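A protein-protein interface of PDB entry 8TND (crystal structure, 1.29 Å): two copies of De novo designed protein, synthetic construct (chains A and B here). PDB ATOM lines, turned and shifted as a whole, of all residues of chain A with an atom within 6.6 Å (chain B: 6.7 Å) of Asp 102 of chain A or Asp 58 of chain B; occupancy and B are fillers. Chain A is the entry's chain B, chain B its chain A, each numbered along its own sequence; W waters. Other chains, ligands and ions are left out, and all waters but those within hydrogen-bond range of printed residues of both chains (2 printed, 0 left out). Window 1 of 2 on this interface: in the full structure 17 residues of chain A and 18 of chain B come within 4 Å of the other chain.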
ATOM      1  N   ALA A  51      -5.237 -12.848   1.534  1.00  0.00           N
ATOM      2  CA  ALA A  51      -5.414 -13.844   0.482  1.00  0.00           C
ATOM      3  C   ALA A  51      -5.669 -15.219   1.079  1.00  0.00           C
ATOM      4  O   ALA A  51      -6.476 -15.994   0.538  1.00  0.00           O
ATOM      5  CB  ALA A  51      -4.208 -13.900  -0.438  1.00  0.00           C
ATOM      6  N   ALA A  97     -14.163 -11.494  -5.826  1.00  0.00           N
ATOM      7  CA  ALA A  97     -13.325 -10.841  -4.828  1.00  0.00           C
ATOM      8  C   ALA A  97     -11.959 -11.498  -4.768  1.00  0.00           C
ATOM      9  O   ALA A  97     -10.928 -10.820  -4.694  1.00  0.00           O
ATOM     10  CB  ALA A  97     -14.015 -10.834  -3.466  1.00  0.00           C
ATOM     11  N   SER A  98     -11.922 -12.822  -4.867  1.00  0.00           N
ATOM     12  CA  SER A  98     -10.657 -13.544  -4.834  1.00  0.00           C
ATOM     13  C   SER A  98      -9.766 -13.165  -6.013  1.00  0.00           C
ATOM     14  O   SER A  98      -8.558 -12.938  -5.854  1.00  0.00           O
ATOM     15  CB  SER A  98     -10.963 -15.035  -4.879  1.00  0.00           C
ATOM     16  OG  SER A  98      -9.910 -15.772  -4.313  1.00  0.00           O
ATOM     17  N   LYS A  99     -10.335 -13.121  -7.206  1.00  0.00           N
ATOM     18  CA  LYS A  99      -9.575 -12.791  -8.405  1.00  0.00           C
ATOM     19  C   LYS A  99      -9.024 -11.374  -8.316  1.00  0.00           C
ATOM     20  O   LYS A  99      -7.873 -11.110  -8.703  1.00  0.00           O
ATOM     21  CB  LYS A  99     -10.502 -12.922  -9.622  1.00  0.00           C
ATOM     22  CG  LYS A  99      -9.933 -12.441 -10.957  1.00  0.00           C
ATOM     23  CD  LYS A  99     -11.012 -12.413 -12.041  1.00  0.00           C
ATOM     24  CE  LYS A  99     -12.142 -11.447 -11.698  1.00  0.00           C
ATOM     25  NZ  LYS A  99     -12.930 -11.034 -12.895  1.00  0.00           N
ATOM     26  N   THR A 100      -9.839 -10.447  -7.838  1.00  0.00           N
ATOM     27  CA  THR A 100      -9.417  -9.055  -7.779  1.00  0.00           C
ATOM     28  C   THR A 100      -8.378  -8.866  -6.693  1.00  0.00           C
ATOM     29  O   THR A 100      -7.403  -8.138  -6.893  1.00  0.00           O
ATOM     30  CB  THR A 100     -10.608  -8.130  -7.574  1.00  0.00           C
ATOM     31  OG1 THR A 100     -11.282  -8.449  -6.369  1.00  0.00           O
ATOM     32  CG2 THR A 100     -11.602  -8.324  -8.686  1.00  0.00           C
ATOM     33  N   LEU A 101      -8.527  -9.538  -5.554  1.00  0.00           N
ATOM     34  CA  LEU A 101      -7.467  -9.496  -4.552  1.00  0.00           C
ATOM     35  C   LEU A 101      -6.170 -10.052  -5.121  1.00  0.00           C
ATOM     36  O   LEU A 101      -5.084  -9.507  -4.872  1.00  0.00           O
ATOM     37  CB  LEU A 101      -7.902 -10.266  -3.309  1.00  0.00           C
ATOM     38  CG  LEU A 101      -6.931 -10.256  -2.128  1.00  0.00           C
ATOM     39  CD1 LEU A 101      -6.616  -8.830  -1.613  1.00  0.00           C
ATOM     40  CD2 LEU A 101      -7.429 -11.141  -1.014  1.00  0.00           C
ATOM     41  N   ASP A 102      -6.233 -11.107  -5.920  1.00  0.00           N
ATOM     42  CA  ASP A 102      -5.016 -11.646  -6.514  1.00  0.00           C
ATOM     43  C   ASP A 102      -4.348 -10.613  -7.407  1.00  0.00           C
ATOM     44  O   ASP A 102      -3.120 -10.440  -7.369  1.00  0.00           O
ATOM     45  CB  ASP A 102      -5.333 -12.893  -7.352  1.00  0.00           C
ATOM     46  CG  ASP A 102      -5.240 -14.203  -6.554  1.00  0.00           C
ATOM     47  OD1 ASP A 102      -4.930 -14.175  -5.347  1.00  0.00           O
ATOM     48  OD2 ASP A 102      -5.469 -15.273  -7.167  1.00  0.00           O
ATOM     49  N   THR A 103      -5.132  -9.912  -8.220  1.00  0.00           N
ATOM     50  CA  THR A 103      -4.602  -8.826  -9.038  1.00  0.00           C
ATOM     51  C   THR A 103      -3.921  -7.773  -8.173  1.00  0.00           C
ATOM     52  O   THR A 103      -2.826  -7.290  -8.507  1.00  0.00           O
ATOM     53  CB  THR A 103      -5.724  -8.216  -9.865  1.00  0.00           C
ATOM     54  OG1 THR A 103      -6.241  -9.210 -10.763  1.00  0.00           O
ATOM     55  CG2 THR A 103      -5.239  -7.012 -10.668  1.00  0.00           C
ATOM     56  N   ALA A 104      -4.522  -7.433  -7.046  1.00  0.00           N
ATOM     57  CA  ALA A 104      -3.924  -6.460  -6.136  1.00  0.00           C
ATOM     58  C   ALA A 104      -2.617  -6.967  -5.557  1.00  0.00           C
ATOM     59  O   ALA A 104      -1.624  -6.235  -5.511  1.00  0.00           O
ATOM     60  CB  ALA A 104      -4.921  -6.088  -5.047  1.00  0.00           C
ATOM     61  N   VAL A 105      -2.577  -8.207  -5.081  1.00  0.00           N
ATOM     62  CA  VAL A 105      -1.356  -8.779  -4.532  1.00  0.00           C
ATOM     63  C   VAL A 105      -0.247  -8.776  -5.568  1.00  0.00           C
ATOM     64  O   VAL A 105       0.901  -8.405  -5.271  1.00  0.00           O
ATOM     65  CB  VAL A 105      -1.639 -10.200  -4.007  1.00  0.00           C
ATOM     66  CG1 VAL A 105      -0.359 -10.866  -3.545  1.00  0.00           C
ATOM     67  CG2 VAL A 105      -2.648 -10.160  -2.887  1.00  0.00           C
ATOM     68  N   ALA A 106      -0.551  -9.158  -6.797  1.00  0.00           N
ATOM     69  CA  ALA A 106       0.475  -9.150  -7.827  1.00  0.00           C
ATOM     70  C   ALA A 106       0.931  -7.727  -8.116  1.00  0.00           C
ATOM     71  O   ALA A 106       2.140  -7.479  -8.306  1.00  0.00           O
ATOM     72  CB  ALA A 106      -0.044  -9.817  -9.094  1.00  0.00           C
ATOM     73  N   ALA A 107       0.006  -6.779  -8.186  1.00  0.00           N
ATOM     74  CA  ALA A 107       0.387  -5.397  -8.481  1.00  0.00           C
ATOM     75  C   ALA A 107       1.270  -4.825  -7.380  1.00  0.00           C
ATOM     76  O   ALA A 107       2.252  -4.119  -7.664  1.00  0.00           O
ATOM     77  CB  ALA A 107      -0.839  -4.529  -8.693  1.00  0.00           C
ATOM     78  N   ALA A 119      -7.575  -2.521  -8.181  1.00  0.00           N
ATOM     79  CA  ALA A 119      -8.005  -3.869  -7.817  1.00  0.00           C
ATOM     80  C   ALA A 119      -8.402  -3.958  -6.349  1.00  0.00           C
ATOM     81  O   ALA A 119      -9.399  -4.613  -6.010  1.00  0.00           O
ATOM     82  CB  ALA A 119      -6.902  -4.864  -8.154  1.00  0.00           C
ATOM     83  N   ALA B  51      -7.657 -26.914  -5.454  1.00  0.00           N
ATOM     84  CA  ALA B  51      -7.769 -25.491  -5.134  1.00  0.00           C
ATOM     85  C   ALA B  51      -6.817 -25.107  -4.008  1.00  0.00           C
ATOM     86  O   ALA B  51      -6.228 -24.010  -4.024  1.00  0.00           O
ATOM     87  CB  ALA B  51      -9.206 -25.148  -4.750  1.00  0.00           C
ATOM     88  N   TYR B  53      -3.886 -26.596  -3.223  1.00  0.00           N
ATOM     89  CA  TYR B  53      -2.536 -26.567  -3.760  1.00  0.00           C
ATOM     90  C   TYR B  53      -2.343 -25.375  -4.680  1.00  0.00           C
ATOM     91  O   TYR B  53      -1.296 -24.719  -4.656  1.00  0.00           O
ATOM     92  CB  TYR B  53      -2.222 -27.838  -4.532  1.00  0.00           C
ATOM     93  CG  TYR B  53      -2.108 -29.060  -3.692  1.00  0.00           C
ATOM     94  CD1 TYR B  53      -1.335 -29.078  -2.525  1.00  0.00           C
ATOM     95  CD2 TYR B  53      -2.763 -30.223  -4.053  1.00  0.00           C
ATOM     96  CE1 TYR B  53      -1.239 -30.240  -1.741  1.00  0.00           C
ATOM     97  CE2 TYR B  53      -2.666 -31.376  -3.287  1.00  0.00           C
ATOM     98  CZ  TYR B  53      -1.904 -31.378  -2.140  1.00  0.00           C
ATOM     99  OH  TYR B  53      -1.805 -32.537  -1.387  1.00  0.00           O
ATOM    100  N   GLN B  54      -3.320 -25.064  -5.505  1.00  0.00           N
ATOM    101  CA  GLN B  54      -3.200 -23.911  -6.374  1.00  0.00           C
ATOM    102  C   GLN B  54      -3.012 -22.634  -5.566  1.00  0.00           C
ATOM    103  O   GLN B  54      -2.226 -21.758  -5.958  1.00  0.00           O
ATOM    104  CB  GLN B  54      -4.424 -23.815  -7.285  1.00  0.00           C
ATOM    105  CG  GLN B  54      -4.427 -22.657  -8.267  1.00  0.00           C
ATOM    106  CD  GLN B  54      -3.347 -22.789  -9.283  1.00  0.00           C
ATOM    107  OE1 GLN B  54      -3.313 -23.728 -10.045  1.00  0.00           O
ATOM    108  NE2 GLN B  54      -2.429 -21.834  -9.313  1.00  0.00           N
ATOM    109  N   SER B  55      -3.736 -22.475  -4.458  1.00  0.00           N
ATOM    110  CA  SER B  55      -3.564 -21.279  -3.634  1.00  0.00           C
ATOM    111  C   SER B  55      -2.147 -21.211  -3.087  1.00  0.00           C
ATOM    112  O   SER B  55      -1.563 -20.117  -2.981  1.00  0.00           O
ATOM    113  CB  SER B  55      -4.595 -21.251  -2.509  1.00  0.00           C
ATOM    114  OG  SER B  55      -5.882 -21.011  -3.038  1.00  0.00           O
ATOM    115  N   GLN B  56      -1.563 -22.355  -2.749  1.00  0.00           N
ATOM    116  CA  GLN B  56      -0.178 -22.379  -2.293  1.00  0.00           C
ATOM    117  C   GLN B  56       0.796 -22.030  -3.411  1.00  0.00           C
ATOM    118  O   GLN B  56       1.768 -21.301  -3.174  1.00  0.00           O
ATOM    119  CB  GLN B  56       0.134 -23.751  -1.702  1.00  0.00           C
ATOM    120  CG  GLN B  56      -0.659 -24.075  -0.443  1.00  0.00           C
ATOM    121  CD  GLN B  56      -0.286 -25.417   0.136  1.00  0.00           C
ATOM    122  OE1 GLN B  56      -0.543 -26.458  -0.464  1.00  0.00           O
ATOM    123  NE2 GLN B  56       0.321 -25.400   1.319  1.00  0.00           N
ATOM    124  N   VAL B  57       0.587 -22.538  -4.623  1.00  0.00           N
ATOM    125  CA  VAL B  57       1.426 -22.142  -5.751  1.00  0.00           C
ATOM    126  C   VAL B  57       1.341 -20.645  -5.949  1.00  0.00           C
ATOM    127  O   VAL B  57       2.364 -19.990  -6.203  1.00  0.00           O
ATOM    128  CB  VAL B  57       1.041 -22.888  -7.045  1.00  0.00           C
ATOM    129  CG1 VAL B  57       1.892 -22.410  -8.207  1.00  0.00           C
ATOM    130  CG2 VAL B  57       1.192 -24.409  -6.884  1.00  0.00           C
ATOM    131  N   ASP B  58       0.151 -20.077  -5.857  1.00  0.00           N
ATOM    132  CA  ASP B  58      -0.054 -18.639  -6.015  1.00  0.00           C
ATOM    133  C   ASP B  58       0.793 -17.875  -5.007  1.00  0.00           C
ATOM    134  O   ASP B  58       1.498 -16.916  -5.351  1.00  0.00           O
ATOM    135  CB  ASP B  58      -1.529 -18.284  -5.731  1.00  0.00           C
ATOM    136  CG  ASP B  58      -2.535 -18.763  -6.787  1.00  0.00           C
ATOM    137  OD1 ASP B  58      -2.153 -19.321  -7.821  1.00  0.00           O
ATOM    138  OD2 ASP B  58      -3.759 -18.623  -6.499  1.00  0.00           O
ATOM    139  N   GLN B  59       0.781 -18.329  -3.754  1.00  0.00           N
ATOM    140  CA  GLN B  59       1.564 -17.687  -2.701  1.00  0.00           C
ATOM    141  C   GLN B  59       3.056 -17.799  -2.987  1.00  0.00           C
ATOM    142  O   GLN B  59       3.795 -16.825  -2.809  1.00  0.00           O
ATOM    143  CB  GLN B  59       1.187 -18.323  -1.362  1.00  0.00           C
ATOM    144  CG  GLN B  59       1.988 -17.794  -0.173  1.00  0.00           C
ATOM    145  CD  GLN B  59       1.788 -16.315   0.093  1.00  0.00           C
ATOM    146  OE1 GLN B  59       0.699 -15.750  -0.116  1.00  0.00           O
ATOM    147  NE2 GLN B  59       2.869 -15.654   0.529  1.00  0.00           N
ATOM    148  N   TYR B  60       3.538 -18.973  -3.381  1.00  0.00           N
ATOM    149  CA  TYR B  60       4.959 -19.114  -3.690  1.00  0.00           C
ATOM    150  C   TYR B  60       5.348 -18.248  -4.868  1.00  0.00           C
ATOM    151  O   TYR B  60       6.456 -17.701  -4.894  1.00  0.00           O
ATOM    152  CB  TYR B  60       5.314 -20.575  -3.982  1.00  0.00           C
ATOM    153  CG  TYR B  60       5.347 -21.503  -2.800  1.00  0.00           C
ATOM    154  CD1 TYR B  60       5.962 -21.156  -1.612  1.00  0.00           C
ATOM    155  CD2 TYR B  60       4.754 -22.757  -2.888  1.00  0.00           C
ATOM    156  CE1 TYR B  60       6.000 -22.039  -0.541  1.00  0.00           C
ATOM    157  CE2 TYR B  60       4.777 -23.628  -1.834  1.00  0.00           C
ATOM    158  CZ  TYR B  60       5.396 -23.272  -0.668  1.00  0.00           C
ATOM    159  OH  TYR B  60       5.394 -24.178   0.382  1.00  0.00           O
ATOM    160  N   ALA B  61       4.491 -18.109  -5.858  1.00  0.00           N
ATOM    161  CA  ALA B  61       4.800 -17.281  -7.015  1.00  0.00           C
ATOM    162  C   ALA B  61       4.890 -15.804  -6.641  1.00  0.00           C
ATOM    163  O   ALA B  61       5.739 -15.068  -7.161  1.00  0.00           O
ATOM    164  CB  ALA B  61       3.748 -17.503  -8.094  1.00  0.00           C
ATOM    165  N   VAL B  62       4.048 -15.361  -5.717  1.00  0.00           N
ATOM    166  CA  VAL B  62       4.121 -14.004  -5.186  1.00  0.00           C
ATOM    167  C   VAL B  62       5.440 -13.809  -4.450  1.00  0.00           C
ATOM    168  O   VAL B  62       6.132 -12.800  -4.630  1.00  0.00           O
ATOM    169  CB  VAL B  62       2.916 -13.743  -4.251  1.00  0.00           C
ATOM    170  CG1 VAL B  62       3.104 -12.464  -3.392  1.00  0.00           C
ATOM    171  CG2 VAL B  62       1.598 -13.689  -5.057  1.00  0.00           C
ATOM    172  N   GLU B  63       5.803 -14.768  -3.609  1.00  0.00           N
ATOM    173  CA  GLU B  63       7.037 -14.686  -2.831  1.00  0.00           C
ATOM    174  C   GLU B  63       8.242 -14.635  -3.751  1.00  0.00           C
ATOM    175  O   GLU B  63       9.222 -13.916  -3.479  1.00  0.00           O
ATOM    176  CB  GLU B  63       7.153 -15.881  -1.884  1.00  0.00           C
ATOM    177  CG  GLU B  63       6.205 -15.824  -0.719  1.00  0.00           C
ATOM    178  CD  GLU B  63       6.241 -17.095   0.115  1.00  0.00           C
ATOM    179  OE1 GLU B  63       7.309 -17.762   0.131  1.00  0.00           O
ATOM    180  OE2 GLU B  63       5.222 -17.400   0.783  1.00  0.00           O
ATOM    181  N   LEU B  91       3.882 -15.447 -12.367  1.00  0.00           N
ATOM    182  CA  LEU B  91       2.818 -15.122 -11.421  1.00  0.00           C
ATOM    183  C   LEU B  91       1.525 -14.794 -12.160  1.00  0.00           C
ATOM    184  O   LEU B  91       0.435 -15.217 -11.747  1.00  0.00           O
ATOM    185  CB  LEU B  91       3.252 -13.960 -10.542  1.00  0.00           C
ATOM    186  CG  LEU B  91       2.191 -13.389  -9.587  1.00  0.00           C
ATOM    187  CD1 LEU B  91       1.636 -14.431  -8.625  1.00  0.00           C
ATOM    188  CD2 LEU B  91       2.769 -12.234  -8.800  1.00  0.00           C
ATOM    189  N   VAL B  94       0.087 -18.166 -13.311  1.00  0.00           N
ATOM    190  CA  VAL B  94      -0.419 -18.888 -12.150  1.00  0.00           C
ATOM    191  C   VAL B  94      -1.747 -18.305 -11.684  1.00  0.00           C
ATOM    192  O   VAL B  94      -2.692 -19.044 -11.371  1.00  0.00           O
ATOM    193  CB  VAL B  94       0.644 -18.860 -11.041  1.00  0.00           C
ATOM    194  CG1 VAL B  94       0.099 -19.311  -9.726  1.00  0.00           C
ATOM    195  CG2 VAL B  94       1.832 -19.719 -11.421  1.00  0.00           C
ATOM    196  N   GLN B  95      -1.857 -16.981 -11.620  1.00  0.00           N
ATOM    197  CA  GLN B  95      -3.117 -16.395 -11.172  1.00  0.00           C
ATOM    198  C   GLN B  95      -4.222 -16.586 -12.201  1.00  0.00           C
ATOM    199  O   GLN B  95      -5.403 -16.703 -11.818  1.00  0.00           O
ATOM    200  CB  GLN B  95      -2.896 -14.928 -10.824  1.00  0.00           C
ATOM    201  CG  GLN B  95      -2.021 -14.739  -9.591  1.00  0.00           C
ATOM    202  CD  GLN B  95      -2.011 -13.310  -9.131  1.00  0.00           C
ATOM    203  OE1 GLN B  95      -2.199 -12.407  -9.932  1.00  0.00           O
ATOM    204  NE2 GLN B  95      -1.782 -13.097  -7.850  1.00  0.00           N
ATOM    205  N   GLU B  96      -3.892 -16.653 -13.485  1.00  0.00           N
ATOM    206  CA  GLU B  96      -4.914 -16.977 -14.474  1.00  0.00           C
ATOM    207  C   GLU B  96      -5.377 -18.416 -14.295  1.00  0.00           C
ATOM    208  O   GLU B  96      -6.579 -18.709 -14.347  1.00  0.00           O
ATOM    209  CB  GLU B  96      -4.409 -16.724 -15.890  1.00  0.00           C
ATOM    210  CG  GLU B  96      -5.533 -16.728 -16.911  1.00  0.00           C
ATOM    211  CD  GLU B  96      -5.052 -16.556 -18.343  1.00  0.00           C
ATOM    212  OE1 GLU B  96      -3.857 -16.238 -18.545  1.00  0.00           O
ATOM    213  OE2 GLU B  96      -5.881 -16.743 -19.263  1.00  0.00           O
ATOM    214  N   ALA B  97      -4.446 -19.319 -14.019  1.00  0.00           N
ATOM    215  CA  ALA B  97      -4.817 -20.696 -13.704  1.00  0.00           C
ATOM    216  C   ALA B  97      -5.707 -20.748 -12.467  1.00  0.00           C
ATOM    217  O   ALA B  97      -6.698 -21.490 -12.432  1.00  0.00           O
ATOM    218  CB  ALA B  97      -3.557 -21.541 -13.514  1.00  0.00           C
ATOM    219  N   SER B  98      -5.403 -19.956 -11.456  1.00  0.00           N
ATOM    220  CA  SER B  98      -6.184 -19.959 -10.230  1.00  0.00           C
ATOM    221  C   SER B  98      -7.622 -19.504 -10.479  1.00  0.00           C
ATOM    222  O   SER B  98      -8.576 -20.115  -9.977  1.00  0.00           O
ATOM    223  CB  SER B  98      -5.480 -19.069  -9.205  1.00  0.00           C
ATOM    224  OG  SER B  98      -6.057 -19.248  -7.942  1.00  0.00           O
ATOM    225  N   LYS B  99      -7.807 -18.450 -11.266  1.00  0.00           N
ATOM    226  CA  LYS B  99      -9.150 -17.945 -11.534  1.00  0.00           C
ATOM    227  C   LYS B  99      -9.933 -18.960 -12.344  1.00  0.00           C
ATOM    228  O   LYS B  99     -11.151 -19.098 -12.181  1.00  0.00           O
ATOM    229  CB  LYS B  99      -9.041 -16.618 -12.303  1.00  0.00           C
ATOM    230  CG  LYS B  99     -10.241 -16.217 -13.181  1.00  0.00           C
ATOM    231  CD  LYS B  99      -9.906 -15.038 -14.092  1.00  0.00           C
ATOM    232  CE  LYS B  99      -9.365 -15.532 -15.441  1.00  0.00           C
ATOM    233  NZ  LYS B  99     -10.376 -15.455 -16.536  1.00  0.00           N
ATOM    234  N   ASP B 102     -11.060 -21.729 -10.191  1.00  0.00           N
ATOM    235  CA  ASP B 102     -12.230 -21.264  -9.449  1.00  0.00           C
ATOM    236  C   ASP B 102     -13.502 -21.433 -10.267  1.00  0.00           C
ATOM    237  O   ASP B 102     -14.522 -21.912  -9.755  1.00  0.00           O
ATOM    238  CB  ASP B 102     -12.083 -19.772  -9.098  1.00  0.00           C
ATOM    239  CG  ASP B 102     -11.246 -19.518  -7.861  1.00  0.00           C
ATOM    240  OD1 ASP B 102     -10.890 -18.321  -7.660  1.00  0.00           O
ATOM    241  OD2 ASP B 102     -10.969 -20.469  -7.089  1.00  0.00           O
HETATM  242  O   HOH W   1      -6.654 -14.866 -10.038  1.00  0.00           O
HETATM  243  O   HOH W   2      -5.466 -17.363  -4.089  1.00  0.00           O
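O of Asp 102 of chain A lies within hydrogen-bond range of NE2 of Gln 95 of chain B (3.0 Å).
The backbone carbonyl oxygen of Lys 99 of chain A is in hydrogen-bond range of the side-chain hydroxyl of Thr 103 of chain A (3.2 Å). The side-chain amide nitrogen (NE2) of Gln 54 of chain B sits at hydrogen-bond distance from the side-chain carboxylate (OD1) of Asp 58 of chain B, 2.9 Å away. The side-chain carboxylate of Asp 58 of chain B sits at hydrogen-bond distance from the side-chain hydroxyl of Ser 98 of chain B (2.8 Å).
Among the printed residues, pairs that only touch across the chains: Lys 99 of chain A with Lys 99 of chain B (3.5 Å), Asp 102 of chain A with Asp 58 of chain B (3.8 Å), Val 105 of chain A with Val 62 of chain B (3.8 Å), Ala 106 of chain A with Leu 91 of chain B (3.7 Å) and Ala 106 of chain A with Gln 95 of chain B (3.5 Å).
Asp 102 of chain A touches just these residues of chain B: Asp 58 (3.8 Å) and Gln 95 (3.0 Å). Of chain A, only Asp 102 (3.8 Å) comes within 4 Å of Asp 58 of chain B. Of the printed residues of chain B, Lys 99 of chain A touches Lys 99. Of the printed residues of chain B, Ala 106 of chain A touches Leu 91 and Gln 95. Ala 104 of chain A touches none of the printed residues of chain B. Asp 102 of chain B touches none of the printed residues of chain A. The nearest residue of chain B that does not touch Asp 102 of chain A is Ser 98 of chain B (4.1 Å). The nearest printed residue of chain A that does not touch Lys 99 of chain B is Asp 102 of chain A (5.7 Å).
Of the 20 printed residues of chain B, 5 touch a printed residue of chain A. Printed residues of chain B that touch a printed residue of chain A: Asp 58, Val 62, Leu 91, Gln 95 and Lys 99. Hydrophobic or aromatic side chains of chain B that line the printed part of chain A: Val 62 and Leu 91. Along chain B the printed residues that touch a printed residue of chain A span positions 58 to 99. Of the 13 printed residues of chain A, 4 touch a printed residue of chain B. Hydrophobic or aromatic side chains of chain A within 4 Å of the printed part of chain B: Val 105 and Ala 106. Among the printed residues, no Asp or Glu carboxylate lies within 4 Å of a Lys or Arg side-chain nitrogen of the other chain.
Lys 99 of chain A touches its own counterpart, Lys 99 of chain B. 5 positions are printed for both chains.
Water W1 bridges the backbone carbonyl oxygen of Gln 95 of chain B and the side-chain carboxylate of Asp 102 of chain A. Water W2 bridges OD2 of Asp 58 of chain B (3.2 Å) and OD1 of Asp 102 of chain A (3.5 Å).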
